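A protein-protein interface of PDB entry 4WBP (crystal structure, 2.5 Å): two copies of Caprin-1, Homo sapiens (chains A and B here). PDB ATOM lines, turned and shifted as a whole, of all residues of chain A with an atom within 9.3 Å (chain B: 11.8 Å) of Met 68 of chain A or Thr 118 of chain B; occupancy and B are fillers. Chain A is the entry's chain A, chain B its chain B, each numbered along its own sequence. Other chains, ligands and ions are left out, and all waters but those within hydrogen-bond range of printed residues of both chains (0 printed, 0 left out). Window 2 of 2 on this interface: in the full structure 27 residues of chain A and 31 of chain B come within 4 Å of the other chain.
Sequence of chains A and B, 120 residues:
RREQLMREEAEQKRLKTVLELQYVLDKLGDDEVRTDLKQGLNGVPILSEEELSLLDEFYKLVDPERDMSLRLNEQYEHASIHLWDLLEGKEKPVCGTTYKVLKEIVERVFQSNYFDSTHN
Hydrophobic or aromatic side chains of chain A within 4 Å of the printed part of chain B: Met 68 and Leu 72. Hydrophobic or aromatic side chains of chain B within 4 Å of the printed part of chain A: Tyr 23, Val 24 and Phe 115. Among the printed residues, 12 pairs touch across the chains. Among the printed residues, Asp or Glu carboxylates within 4 Å of a Lys or Arg side-chain nitrogen of the other chain: Arg 71 of chain A with Asp 116 of chain B.
Among the printed residues, pairs that only touch across the chains: Met 68 of chain A with Asp 116 of chain B (3.2 Å), Arg 66 of chain A with Tyr 23 of chain B (3.4 Å), Met 68 of chain A with Ser 117 of chain B (3.4 Å), Leu 72 of chain A with Tyr 23 of chain B (3.5 Å), Met 68 of chain A with Thr 118 of chain B (3.6 Å), Met 68 of chain A with Phe 115 of chain B (3.7 Å), Leu 72 of chain A with Val 24 of chain B (3.8 Å) and Leu 72 of chain A with Phe 115 of chain B (3.96 Å).
Printed residues of chain B within 4 Å of Arg 66 of chain A: Tyr 23 and Phe 115. No residue of chain B comes within 4 Å of Asp 67 of chain A. Of chain B, only Phe 115 (3.7 Å), Asp 116 (3.2 Å), Ser 117 (3.4 Å) and Thr 118 (3.6 Å) come within 4 Å of Met 68 of chain A. No residue of chain B comes within 4 Å of Ser 69 of chain A. No residue of chain B comes within 4 Å of Leu 70 of chain A. Printed residues of chain B within 4 Å of Arg 71 of chain A: Asn 113 (3.1 Å) and Asp 116 (3.4 Å). Of the printed residues of chain A, Phe 115 of chain B touches Arg 66 (2.9 Å), Met 68 (3.7 Å) and Leu 72 (3.96 Å). Of chain A, only Met 68 comes within 4 Å of Ser 117 of chain B. Of the printed residues of chain A, Thr 118 of chain B touches Met 68. No residue of chain A comes within 4 Å of His 119 of chain B. The nearest residue of chain B that does not touch Met 68 of chain A is Tyr 23 of chain B (5.3 Å). The nearest residue of chain A that does not touch Thr 118 of chain B is Arg 66 of chain A (7.4 Å).
ND2 of Asn 113 of chain B sits close to NH2 of Arg 71 of chain A (3.1 Å). NE of Arg 71 of chain A is in salt-bridge range of OD2 of Asp 116 of chain B (3.4 Å). O of Phe 115 of chain B lies within hydrogen-bond range of NH2 of Arg 66 of chain A (2.9 Å). N of Leu 72 of chain A is in hydrogen-bond range of OD1 of Asp 116 of chain B, at 3.0 Å.
The backbone carbonyl oxygen of Leu 70 of chain A is in hydrogen-bond range of the guanidinium group of Arg 66 of chain A (3.1 Å). The guanidinium group of Arg 66 of chain A is in hydrogen-bond range of the side-chain amide oxygen of Gln 75 of chain A (2.9 Å). The backbone NH (N) of Arg 71 of chain A lies within hydrogen-bond range of the side-chain carboxylate (OE1) of Glu 74 of chain A (2.7 Å). ND2 of Asn 113 of chain B is in hydrogen-bond range of OD2 of Asp 116 of chain B, 2.8 Å away.
No position is printed for both chains.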
ATOM      1  N   GLU A  65      11.508   4.179  -1.998  1.00  0.00           N
ATOM      2  CA  GLU A  65      11.511   4.466  -0.572  1.00  0.00           C
ATOM      3  C   GLU A  65      11.005   5.885  -0.359  1.00  0.00           C
ATOM      4  O   GLU A  65      11.342   6.789  -1.120  1.00  0.00           O
ATOM      5  CB  GLU A  65      12.931   4.348  -0.020  1.00  0.00           C
ATOM      6  CG  GLU A  65      13.533   2.954  -0.146  1.00  0.00           C
ATOM      7  CD  GLU A  65      15.006   2.914   0.224  1.00  0.00           C
ATOM      8  OE1 GLU A  65      15.598   3.988   0.461  1.00  0.00           O
ATOM      9  OE2 GLU A  65      15.569   1.799   0.276  1.00  0.00           O
ATOM     10  N   ARG A  66      10.199   6.078   0.680  1.00  0.00           N
ATOM     11  CA  ARG A  66       9.646   7.396   0.978  1.00  0.00           C
ATOM     12  C   ARG A  66      10.722   8.441   1.281  1.00  0.00           C
ATOM     13  O   ARG A  66      11.488   8.297   2.235  1.00  0.00           O
ATOM     14  CB  ARG A  66       8.664   7.300   2.148  1.00  0.00           C
ATOM     15  CG  ARG A  66       7.957   8.602   2.485  1.00  0.00           C
ATOM     16  CD  ARG A  66       6.902   8.949   1.445  1.00  0.00           C
ATOM     17  NE  ARG A  66       6.186  10.173   1.791  1.00  0.00           N
ATOM     18  CZ  ARG A  66       6.487  11.376   1.311  1.00  0.00           C
ATOM     19  NH1 ARG A  66       7.488  11.518   0.454  1.00  0.00           N
ATOM     20  NH2 ARG A  66       5.784  12.434   1.684  1.00  0.00           N
ATOM     21  N   ASP A  67      10.769   9.489   0.463  1.00  0.00           N
ATOM     22  CA  ASP A  67      11.666  10.620   0.679  1.00  0.00           C
ATOM     23  C   ASP A  67      10.829  11.787   1.192  1.00  0.00           C
ATOM     24  O   ASP A  67       9.929  12.255   0.497  1.00  0.00           O
ATOM     25  CB  ASP A  67      12.357  10.997  -0.634  1.00  0.00           C
ATOM     26  CG  ASP A  67      13.370  12.122  -0.475  1.00  0.00           C
ATOM     27  OD1 ASP A  67      13.363  12.820   0.560  1.00  0.00           O
ATOM     28  OD2 ASP A  67      14.177  12.317  -1.409  1.00  0.00           O
ATOM     29  N   MET A  68      11.130  12.270   2.393  1.00  0.00           N
ATOM     30  CA  MET A  68      10.328  13.336   2.989  1.00  0.00           C
ATOM     31  C   MET A  68      10.543  14.699   2.332  1.00  0.00           C
ATOM     32  O   MET A  68       9.750  15.619   2.536  1.00  0.00           O
ATOM     33  CB  MET A  68      10.550  13.419   4.502  1.00  0.00           C
ATOM     34  CG  MET A  68      10.044  12.201   5.257  1.00  0.00           C
ATOM     35  SD  MET A  68       8.288  11.596   4.633  1.00  0.00           S
ATOM     36  CE  MET A  68       7.187  13.099   5.210  1.00  0.00           C
ATOM     37  N   SER A  69      11.604  14.828   1.542  1.00  0.00           N
ATOM     38  CA  SER A  69      11.852  16.069   0.811  1.00  0.00           C
ATOM     39  C   SER A  69      10.766  16.296  -0.239  1.00  0.00           C
ATOM     40  O   SER A  69      10.509  17.427  -0.651  1.00  0.00           O
ATOM     41  CB  SER A  69      13.237  16.057   0.159  1.00  0.00           C
ATOM     42  OG  SER A  69      13.309  15.098  -0.881  1.00  0.00           O
ATOM     43  N   LEU A  70      10.136  15.206  -0.665  1.00  0.00           N
ATOM     44  CA  LEU A  70       9.068  15.254  -1.656  1.00  0.00           C
ATOM     45  C   LEU A  70       7.715  15.217  -0.957  1.00  0.00           C
ATOM     46  O   LEU A  70       7.567  14.574   0.081  1.00  0.00           O
ATOM     47  CB  LEU A  70       9.175  14.075  -2.627  1.00  0.00           C
ATOM     48  CG  LEU A  70      10.447  13.953  -3.465  1.00  0.00           C
ATOM     49  CD1 LEU A  70      10.376  12.722  -4.356  1.00  0.00           C
ATOM     50  CD2 LEU A  70      10.658  15.208  -4.296  1.00  0.00           C
ATOM     51  N   ARG A  71       6.726  15.901  -1.525  1.00  0.00           N
ATOM     52  CA  ARG A  71       5.360  15.759  -1.045  1.00  0.00           C
ATOM     53  C   ARG A  71       4.853  14.382  -1.439  1.00  0.00           C
ATOM     54  O   ARG A  71       5.441  13.725  -2.299  1.00  0.00           O
ATOM     55  CB  ARG A  71       4.445  16.820  -1.657  1.00  0.00           C
ATOM     56  CG  ARG A  71       4.421  18.140  -0.913  1.00  0.00           C
ATOM     57  CD  ARG A  71       3.456  19.121  -1.564  1.00  0.00           C
ATOM     58  NE  ARG A  71       2.067  18.776  -1.275  1.00  0.00           N
ATOM     59  CZ  ARG A  71       1.040  19.606  -1.424  1.00  0.00           C
ATOM     60  NH1 ARG A  71       1.242  20.844  -1.857  1.00  0.00           N
ATOM     61  NH2 ARG A  71      -0.190  19.204  -1.133  1.00  0.00           N
ATOM     62  N   LEU A  72       3.768  13.943  -0.813  1.00  0.00           N
ATOM     63  CA  LEU A  72       3.203  12.638  -1.133  1.00  0.00           C
ATOM     64  C   LEU A  72       2.751  12.624  -2.587  1.00  0.00           C
ATOM     65  O   LEU A  72       2.900  11.621  -3.285  1.00  0.00           O
ATOM     66  CB  LEU A  72       2.044  12.293  -0.198  1.00  0.00           C
ATOM     67  CG  LEU A  72       1.353  10.964  -0.506  1.00  0.00           C
ATOM     68  CD1 LEU A  72       2.338   9.817  -0.365  1.00  0.00           C
ATOM     69  CD2 LEU A  72       0.150  10.755   0.400  1.00  0.00           C
ATOM     70  N   GLU A  74       4.153  14.072  -4.905  1.00  0.00           N
ATOM     71  CA  GLU A  74       5.344  14.183  -5.744  1.00  0.00           C
ATOM     72  C   GLU A  74       6.105  12.860  -5.780  1.00  0.00           C
ATOM     73  O   GLU A  74       6.852  12.586  -6.719  1.00  0.00           O
ATOM     74  CB  GLU A  74       6.277  15.289  -5.241  1.00  0.00           C
ATOM     75  CG  GLU A  74       5.700  16.696  -5.277  1.00  0.00           C
ATOM     76  CD  GLU A  74       6.657  17.728  -4.696  1.00  0.00           C
ATOM     77  OE1 GLU A  74       7.271  17.445  -3.646  1.00  0.00           O
ATOM     78  OE2 GLU A  74       6.796  18.819  -5.289  1.00  0.00           O
ATOM     79  N   GLN A  75       5.912  12.053  -4.740  1.00  0.00           N
ATOM     80  CA  GLN A  75       6.672  10.823  -4.533  1.00  0.00           C
ATOM     81  C   GLN A  75       6.564   9.810  -5.675  1.00  0.00           C
ATOM     82  O   GLN A  75       7.544   9.149  -6.021  1.00  0.00           O
ATOM     83  CB  GLN A  75       6.234  10.155  -3.225  1.00  0.00           C
ATOM     84  CG  GLN A  75       7.032   8.912  -2.847  1.00  0.00           C
ATOM     85  CD  GLN A  75       8.478   9.218  -2.510  1.00  0.00           C
ATOM     86  OE1 GLN A  75       8.771   9.820  -1.477  1.00  0.00           O
ATOM     87  NE2 GLN A  75       9.391   8.810  -3.385  1.00  0.00           N
ATOM     88  N   TYR B  23      -0.137   3.875  -0.703  1.00  0.00           N
ATOM     89  CA  TYR B  23       0.732   4.318   0.381  1.00  0.00           C
ATOM     90  C   TYR B  23      -0.087   4.669   1.624  1.00  0.00           C
ATOM     91  O   TYR B  23       0.200   4.187   2.722  1.00  0.00           O
ATOM     92  CB  TYR B  23       1.575   5.517  -0.054  1.00  0.00           C
ATOM     93  CG  TYR B  23       2.538   6.006   1.007  1.00  0.00           C
ATOM     94  CD1 TYR B  23       3.773   5.396   1.178  1.00  0.00           C
ATOM     95  CD2 TYR B  23       2.210   7.068   1.842  1.00  0.00           C
ATOM     96  CE1 TYR B  23       4.659   5.831   2.142  1.00  0.00           C
ATOM     97  CE2 TYR B  23       3.091   7.511   2.812  1.00  0.00           C
ATOM     98  CZ  TYR B  23       4.314   6.888   2.956  1.00  0.00           C
ATOM     99  OH  TYR B  23       5.199   7.321   3.919  1.00  0.00           O
ATOM    100  N   VAL B  24      -1.106   5.508   1.447  1.00  0.00           N
ATOM    101  CA  VAL B  24      -1.945   5.934   2.570  1.00  0.00           C
ATOM    102  C   VAL B  24      -2.641   4.771   3.276  1.00  0.00           C
ATOM    103  O   VAL B  24      -2.566   4.643   4.499  1.00  0.00           O
ATOM    104  CB  VAL B  24      -3.008   6.959   2.127  1.00  0.00           C
ATOM    105  CG1 VAL B  24      -4.038   7.164   3.227  1.00  0.00           C
ATOM    106  CG2 VAL B  24      -2.348   8.275   1.756  1.00  0.00           C
ATOM    107  N   LYS B  27      -0.347   2.886   5.273  1.00  0.00           N
ATOM    108  CA  LYS B  27      -0.013   3.569   6.521  1.00  0.00           C
ATOM    109  C   LYS B  27      -1.148   3.533   7.541  1.00  0.00           C
ATOM    110  O   LYS B  27      -0.918   3.695   8.740  1.00  0.00           O
ATOM    111  CB  LYS B  27       0.365   5.025   6.241  1.00  0.00           C
ATOM    112  CG  LYS B  27       1.677   5.194   5.501  1.00  0.00           C
ATOM    113  CD  LYS B  27       2.840   4.666   6.317  1.00  0.00           C
ATOM    114  CE  LYS B  27       4.096   4.563   5.472  1.00  0.00           C
ATOM    115  NZ  LYS B  27       5.288   4.210   6.287  1.00  0.00           N
ATOM    116  N   ASP B  30      -1.067   1.484  10.792  1.00  0.00           N
ATOM    117  CA  ASP B  30      -0.327   1.923  11.984  1.00  0.00           C
ATOM    118  C   ASP B  30      -1.243   2.621  12.993  1.00  0.00           C
ATOM    119  O   ASP B  30      -2.018   3.505  12.629  1.00  0.00           O
ATOM    120  CB  ASP B  30       0.827   2.858  11.600  1.00  0.00           C
ATOM    121  CG  ASP B  30       1.894   2.165  10.764  1.00  0.00           C
ATOM    122  OD1 ASP B  30       1.749   0.955  10.465  1.00  0.00           O
ATOM    123  OD2 ASP B  30       2.897   2.826  10.426  1.00  0.00           O
ATOM    124  N   GLU B  32      -0.469   4.641  15.431  1.00  0.00           N
ATOM    125  CA  GLU B  32      -0.096   6.043  15.584  1.00  0.00           C
ATOM    126  C   GLU B  32      -0.759   6.900  14.525  1.00  0.00           C
ATOM    127  O   GLU B  32      -1.321   7.949  14.823  1.00  0.00           O
ATOM    128  CB  GLU B  32       1.411   6.225  15.461  1.00  0.00           C
ATOM    129  CG  GLU B  32       2.235   5.437  16.453  1.00  0.00           C
ATOM    130  CD  GLU B  32       3.718   5.633  16.218  1.00  0.00           C
ATOM    131  OE1 GLU B  32       4.080   6.534  15.430  1.00  0.00           O
ATOM    132  OE2 GLU B  32       4.523   4.888  16.815  1.00  0.00           O
ATOM    133  N   VAL B  33      -0.663   6.450  13.278  1.00  0.00           N
ATOM    134  CA  VAL B  33      -1.268   7.151  12.155  1.00  0.00           C
ATOM    135  C   VAL B  33      -2.769   7.264  12.381  1.00  0.00           C
ATOM    136  O   VAL B  33      -3.353   8.342  12.237  1.00  0.00           O
ATOM    137  CB  VAL B  33      -0.990   6.426  10.823  1.00  0.00           C
ATOM    138  CG1 VAL B  33      -1.760   7.086   9.689  1.00  0.00           C
ATOM    139  CG2 VAL B  33       0.507   6.416  10.522  1.00  0.00           C
ATOM    140  N   ASP B  36      -3.524   9.728  15.299  1.00  0.00           N
ATOM    141  CA  ASP B  36      -3.171  11.069  14.839  1.00  0.00           C
ATOM    142  C   ASP B  36      -4.162  11.617  13.822  1.00  0.00           C
ATOM    143  O   ASP B  36      -4.302  12.830  13.675  1.00  0.00           O
ATOM    144  CB  ASP B  36      -1.776  11.067  14.213  1.00  0.00           C
ATOM    145  CG  ASP B  36      -0.674  10.899  15.236  1.00  0.00           C
ATOM    146  OD1 ASP B  36      -0.927  11.128  16.437  1.00  0.00           O
ATOM    147  OD2 ASP B  36       0.448  10.530  14.832  1.00  0.00           O
ATOM    148  N   LEU B  37      -4.822  10.721  13.097  1.00  0.00           N
ATOM    149  CA  LEU B  37      -5.827  11.125  12.123  1.00  0.00           C
ATOM    150  C   LEU B  37      -7.205  11.195  12.770  1.00  0.00           C
ATOM    151  O   LEU B  37      -8.071  11.960  12.340  1.00  0.00           O
ATOM    152  CB  LEU B  37      -5.850  10.140  10.956  1.00  0.00           C
ATOM    153  CG  LEU B  37      -4.752  10.350   9.914  1.00  0.00           C
ATOM    154  CD1 LEU B  37      -4.931   9.405   8.736  1.00  0.00           C
ATOM    155  CD2 LEU B  37      -4.715  11.798   9.457  1.00  0.00           C
ATOM    156  N   GLN B  39      -7.663  12.049  15.956  1.00  0.00           N
ATOM    157  CA  GLN B  39      -7.584  13.374  16.551  1.00  0.00           C
ATOM    158  C   GLN B  39      -7.152  14.284  15.417  1.00  0.00           C
ATOM    159  O   GLN B  39      -6.679  13.804  14.391  1.00  0.00           O
ATOM    160  CB  GLN B  39      -6.560  13.427  17.684  1.00  0.00           C
ATOM    161  CG  GLN B  39      -5.136  13.139  17.248  1.00  0.00           C
ATOM    162  CD  GLN B  39      -4.125  13.390  18.350  1.00  0.00           C
ATOM    163  OE1 GLN B  39      -4.344  14.222  19.232  1.00  0.00           O
ATOM    164  NE2 GLN B  39      -3.011  12.669  18.307  1.00  0.00           N
ATOM    165  N   GLY B  40      -7.331  15.588  15.563  1.00  0.00           N
ATOM    166  CA  GLY B  40      -6.877  16.484  14.520  1.00  0.00           C
ATOM    167  C   GLY B  40      -5.419  16.834  14.704  1.00  0.00           C
ATOM    168  O   GLY B  40      -4.630  16.030  15.203  1.00  0.00           O
ATOM    169  N   LEU B  41      -5.053  18.043  14.305  1.00  0.00           N
ATOM    170  CA  LEU B  41      -3.745  18.572  14.646  1.00  0.00           C
ATOM    171  C   LEU B  41      -3.905  19.437  15.891  1.00  0.00           C
ATOM    172  O   LEU B  41      -2.931  19.886  16.488  1.00  0.00           O
ATOM    173  CB  LEU B  41      -3.138  19.326  13.459  1.00  0.00           C
ATOM    174  CG  LEU B  41      -3.872  20.513  12.837  1.00  0.00           C
ATOM    175  CD1 LEU B  41      -3.244  21.832  13.275  1.00  0.00           C
ATOM    176  CD2 LEU B  41      -3.925  20.391  11.313  1.00  0.00           C
ATOM    177  N   PHE B 110      -5.711  13.313   1.984  1.00  0.00           N
ATOM    178  CA  PHE B 110      -4.673  13.867   1.121  1.00  0.00           C
ATOM    179  C   PHE B 110      -4.408  15.340   1.424  1.00  0.00           C
ATOM    180  O   PHE B 110      -3.258  15.767   1.508  1.00  0.00           O
ATOM    181  CB  PHE B 110      -5.079  13.742  -0.351  1.00  0.00           C
ATOM    182  CG  PHE B 110      -4.853  12.378  -0.943  1.00  0.00           C
ATOM    183  CD1 PHE B 110      -4.094  11.430  -0.281  1.00  0.00           C
ATOM    184  CD2 PHE B 110      -5.388  12.055  -2.183  1.00  0.00           C
ATOM    185  CE1 PHE B 110      -3.884  10.179  -0.835  1.00  0.00           C
ATOM    186  CE2 PHE B 110      -5.179  10.808  -2.743  1.00  0.00           C
ATOM    187  CZ  PHE B 110      -4.427   9.869  -2.068  1.00  0.00           C
ATOM    188  N   SER B 112      -5.060  17.080   4.091  1.00  0.00           N
ATOM    189  CA  SER B 112      -4.651  17.366   5.460  1.00  0.00           C
ATOM    190  C   SER B 112      -3.149  17.601   5.501  1.00  0.00           C
ATOM    191  O   SER B 112      -2.639  18.253   6.413  1.00  0.00           O
ATOM    192  CB  SER B 112      -5.030  16.214   6.394  1.00  0.00           C
ATOM    193  OG  SER B 112      -4.128  15.128   6.263  1.00  0.00           O
ATOM    194  N   ASN B 113      -2.452  17.037   4.514  1.00  0.00           N
ATOM    195  CA  ASN B 113      -0.995  17.120   4.403  1.00  0.00           C
ATOM    196  C   ASN B 113      -0.294  16.412   5.552  1.00  0.00           C
ATOM    197  O   ASN B 113       0.868  16.688   5.854  1.00  0.00           O
ATOM    198  CB  ASN B 113      -0.515  18.569   4.278  1.00  0.00           C
ATOM    199  CG  ASN B 113      -1.112  19.276   3.080  1.00  0.00           C
ATOM    200  OD1 ASN B 113      -1.944  20.173   3.223  1.00  0.00           O
ATOM    201  ND2 ASN B 113      -0.692  18.872   1.887  1.00  0.00           N
ATOM    202  N   TYR B 114      -1.015  15.492   6.183  1.00  0.00           N
ATOM    203  CA  TYR B 114      -0.480  14.701   7.278  1.00  0.00           C
ATOM    204  C   TYR B 114       0.749  13.926   6.821  1.00  0.00           C
ATOM    205  O   TYR B 114       1.726  13.806   7.559  1.00  0.00           O
ATOM    206  CB  TYR B 114      -1.548  13.738   7.805  1.00  0.00           C
ATOM    207  CG  TYR B 114      -1.060  12.817   8.901  1.00  0.00           C
ATOM    208  CD1 TYR B 114      -1.098  13.214  10.230  1.00  0.00           C
ATOM    209  CD2 TYR B 114      -0.566  11.552   8.607  1.00  0.00           C
ATOM    210  CE1 TYR B 114      -0.657  12.379  11.236  1.00  0.00           C
ATOM    211  CE2 TYR B 114      -0.117  10.711   9.607  1.00  0.00           C
ATOM    212  CZ  TYR B 114      -0.166  11.129  10.920  1.00  0.00           C
ATOM    213  OH  TYR B 114       0.279  10.293  11.919  1.00  0.00           O
ATOM    214  N   PHE B 115       0.701  13.413   5.595  1.00  0.00           N
ATOM    215  CA  PHE B 115       1.789  12.587   5.084  1.00  0.00           C
ATOM    216  C   PHE B 115       2.897  13.387   4.404  1.00  0.00           C
ATOM    217  O   PHE B 115       3.799  12.809   3.799  1.00  0.00           O
ATOM    218  CB  PHE B 115       1.242  11.520   4.133  1.00  0.00           C
ATOM    219  CG  PHE B 115       0.310  10.544   4.791  1.00  0.00           C
ATOM    220  CD1 PHE B 115      -1.062  10.705   4.698  1.00  0.00           C
ATOM    221  CD2 PHE B 115       0.809   9.474   5.515  1.00  0.00           C
ATOM    222  CE1 PHE B 115      -1.921   9.809   5.309  1.00  0.00           C
ATOM    223  CE2 PHE B 115      -0.044   8.576   6.126  1.00  0.00           C
ATOM    224  CZ  PHE B 115      -1.410   8.743   6.024  1.00  0.00           C
ATOM    225  N   ASP B 116       2.820  14.712   4.484  1.00  0.00           N
ATOM    226  CA  ASP B 116       3.913  15.562   4.019  1.00  0.00           C
ATOM    227  C   ASP B 116       4.891  15.831   5.159  1.00  0.00           C
ATOM    228  O   ASP B 116       6.078  16.079   4.939  1.00  0.00           O
ATOM    229  CB  ASP B 116       3.376  16.879   3.453  1.00  0.00           C
ATOM    230  CG  ASP B 116       2.637  16.694   2.139  1.00  0.00           C
ATOM    231  OD1 ASP B 116       2.950  15.734   1.405  1.00  0.00           O
ATOM    232  OD2 ASP B 116       1.745  17.515   1.838  1.00  0.00           O
ATOM    233  N   SER B 117       4.364  15.797   6.378  1.00  0.00           N
ATOM    234  CA  SER B 117       5.146  15.946   7.601  1.00  0.00           C
ATOM    235  C   SER B 117       5.509  14.606   8.238  1.00  0.00           C
ATOM    236  O   SER B 117       5.003  13.561   7.836  1.00  0.00           O
ATOM    237  CB  SER B 117       4.393  16.815   8.609  1.00  0.00           C
ATOM    238  OG  SER B 117       5.124  16.937   9.817  1.00  0.00           O
ATOM    239  N   THR B 118       6.383  14.649   9.241  1.00  0.00           N
ATOM    240  CA  THR B 118       6.731  13.462  10.017  1.00  0.00           C
ATOM    241  C   THR B 118       6.300  13.672  11.461  1.00  0.00           C
ATOM    242  O   THR B 118       6.299  14.796  11.964  1.00  0.00           O
ATOM    243  CB  THR B 118       8.235  13.145   9.958  1.00  0.00           C
ATOM    244  OG1 THR B 118       8.986  14.320  10.284  1.00  0.00           O
ATOM    245  CG2 THR B 118       8.624  12.675   8.571  1.00  0.00           C
ATOM    246  N   HIS B 119       5.928  12.583  12.124  1.00  0.00           N
ATOM    247  CA  HIS B 119       5.303  12.673  13.435  1.00  0.00           C
ATOM    248  C   HIS B 119       5.930  11.701  14.427  1.00  0.00           C
ATOM    249  O   HIS B 119       6.613  12.112  15.365  1.00  0.00           O
ATOM    250  CB  HIS B 119       3.815  12.370  13.278  1.00  0.00           C
ATOM    251  CG  HIS B 119       3.130  13.253  12.281  1.00  0.00           C
ATOM    252  ND1 HIS B 119       3.114  14.625  12.384  1.00  0.00           N
ATOM    253  CD2 HIS B 119       2.486  12.955  11.126  1.00  0.00           C
ATOM    254  CE1 HIS B 119       2.458  15.135  11.357  1.00  0.00           C
ATOM    255  NE2 HIS B 119       2.067  14.144  10.579  1.00  0.00           N
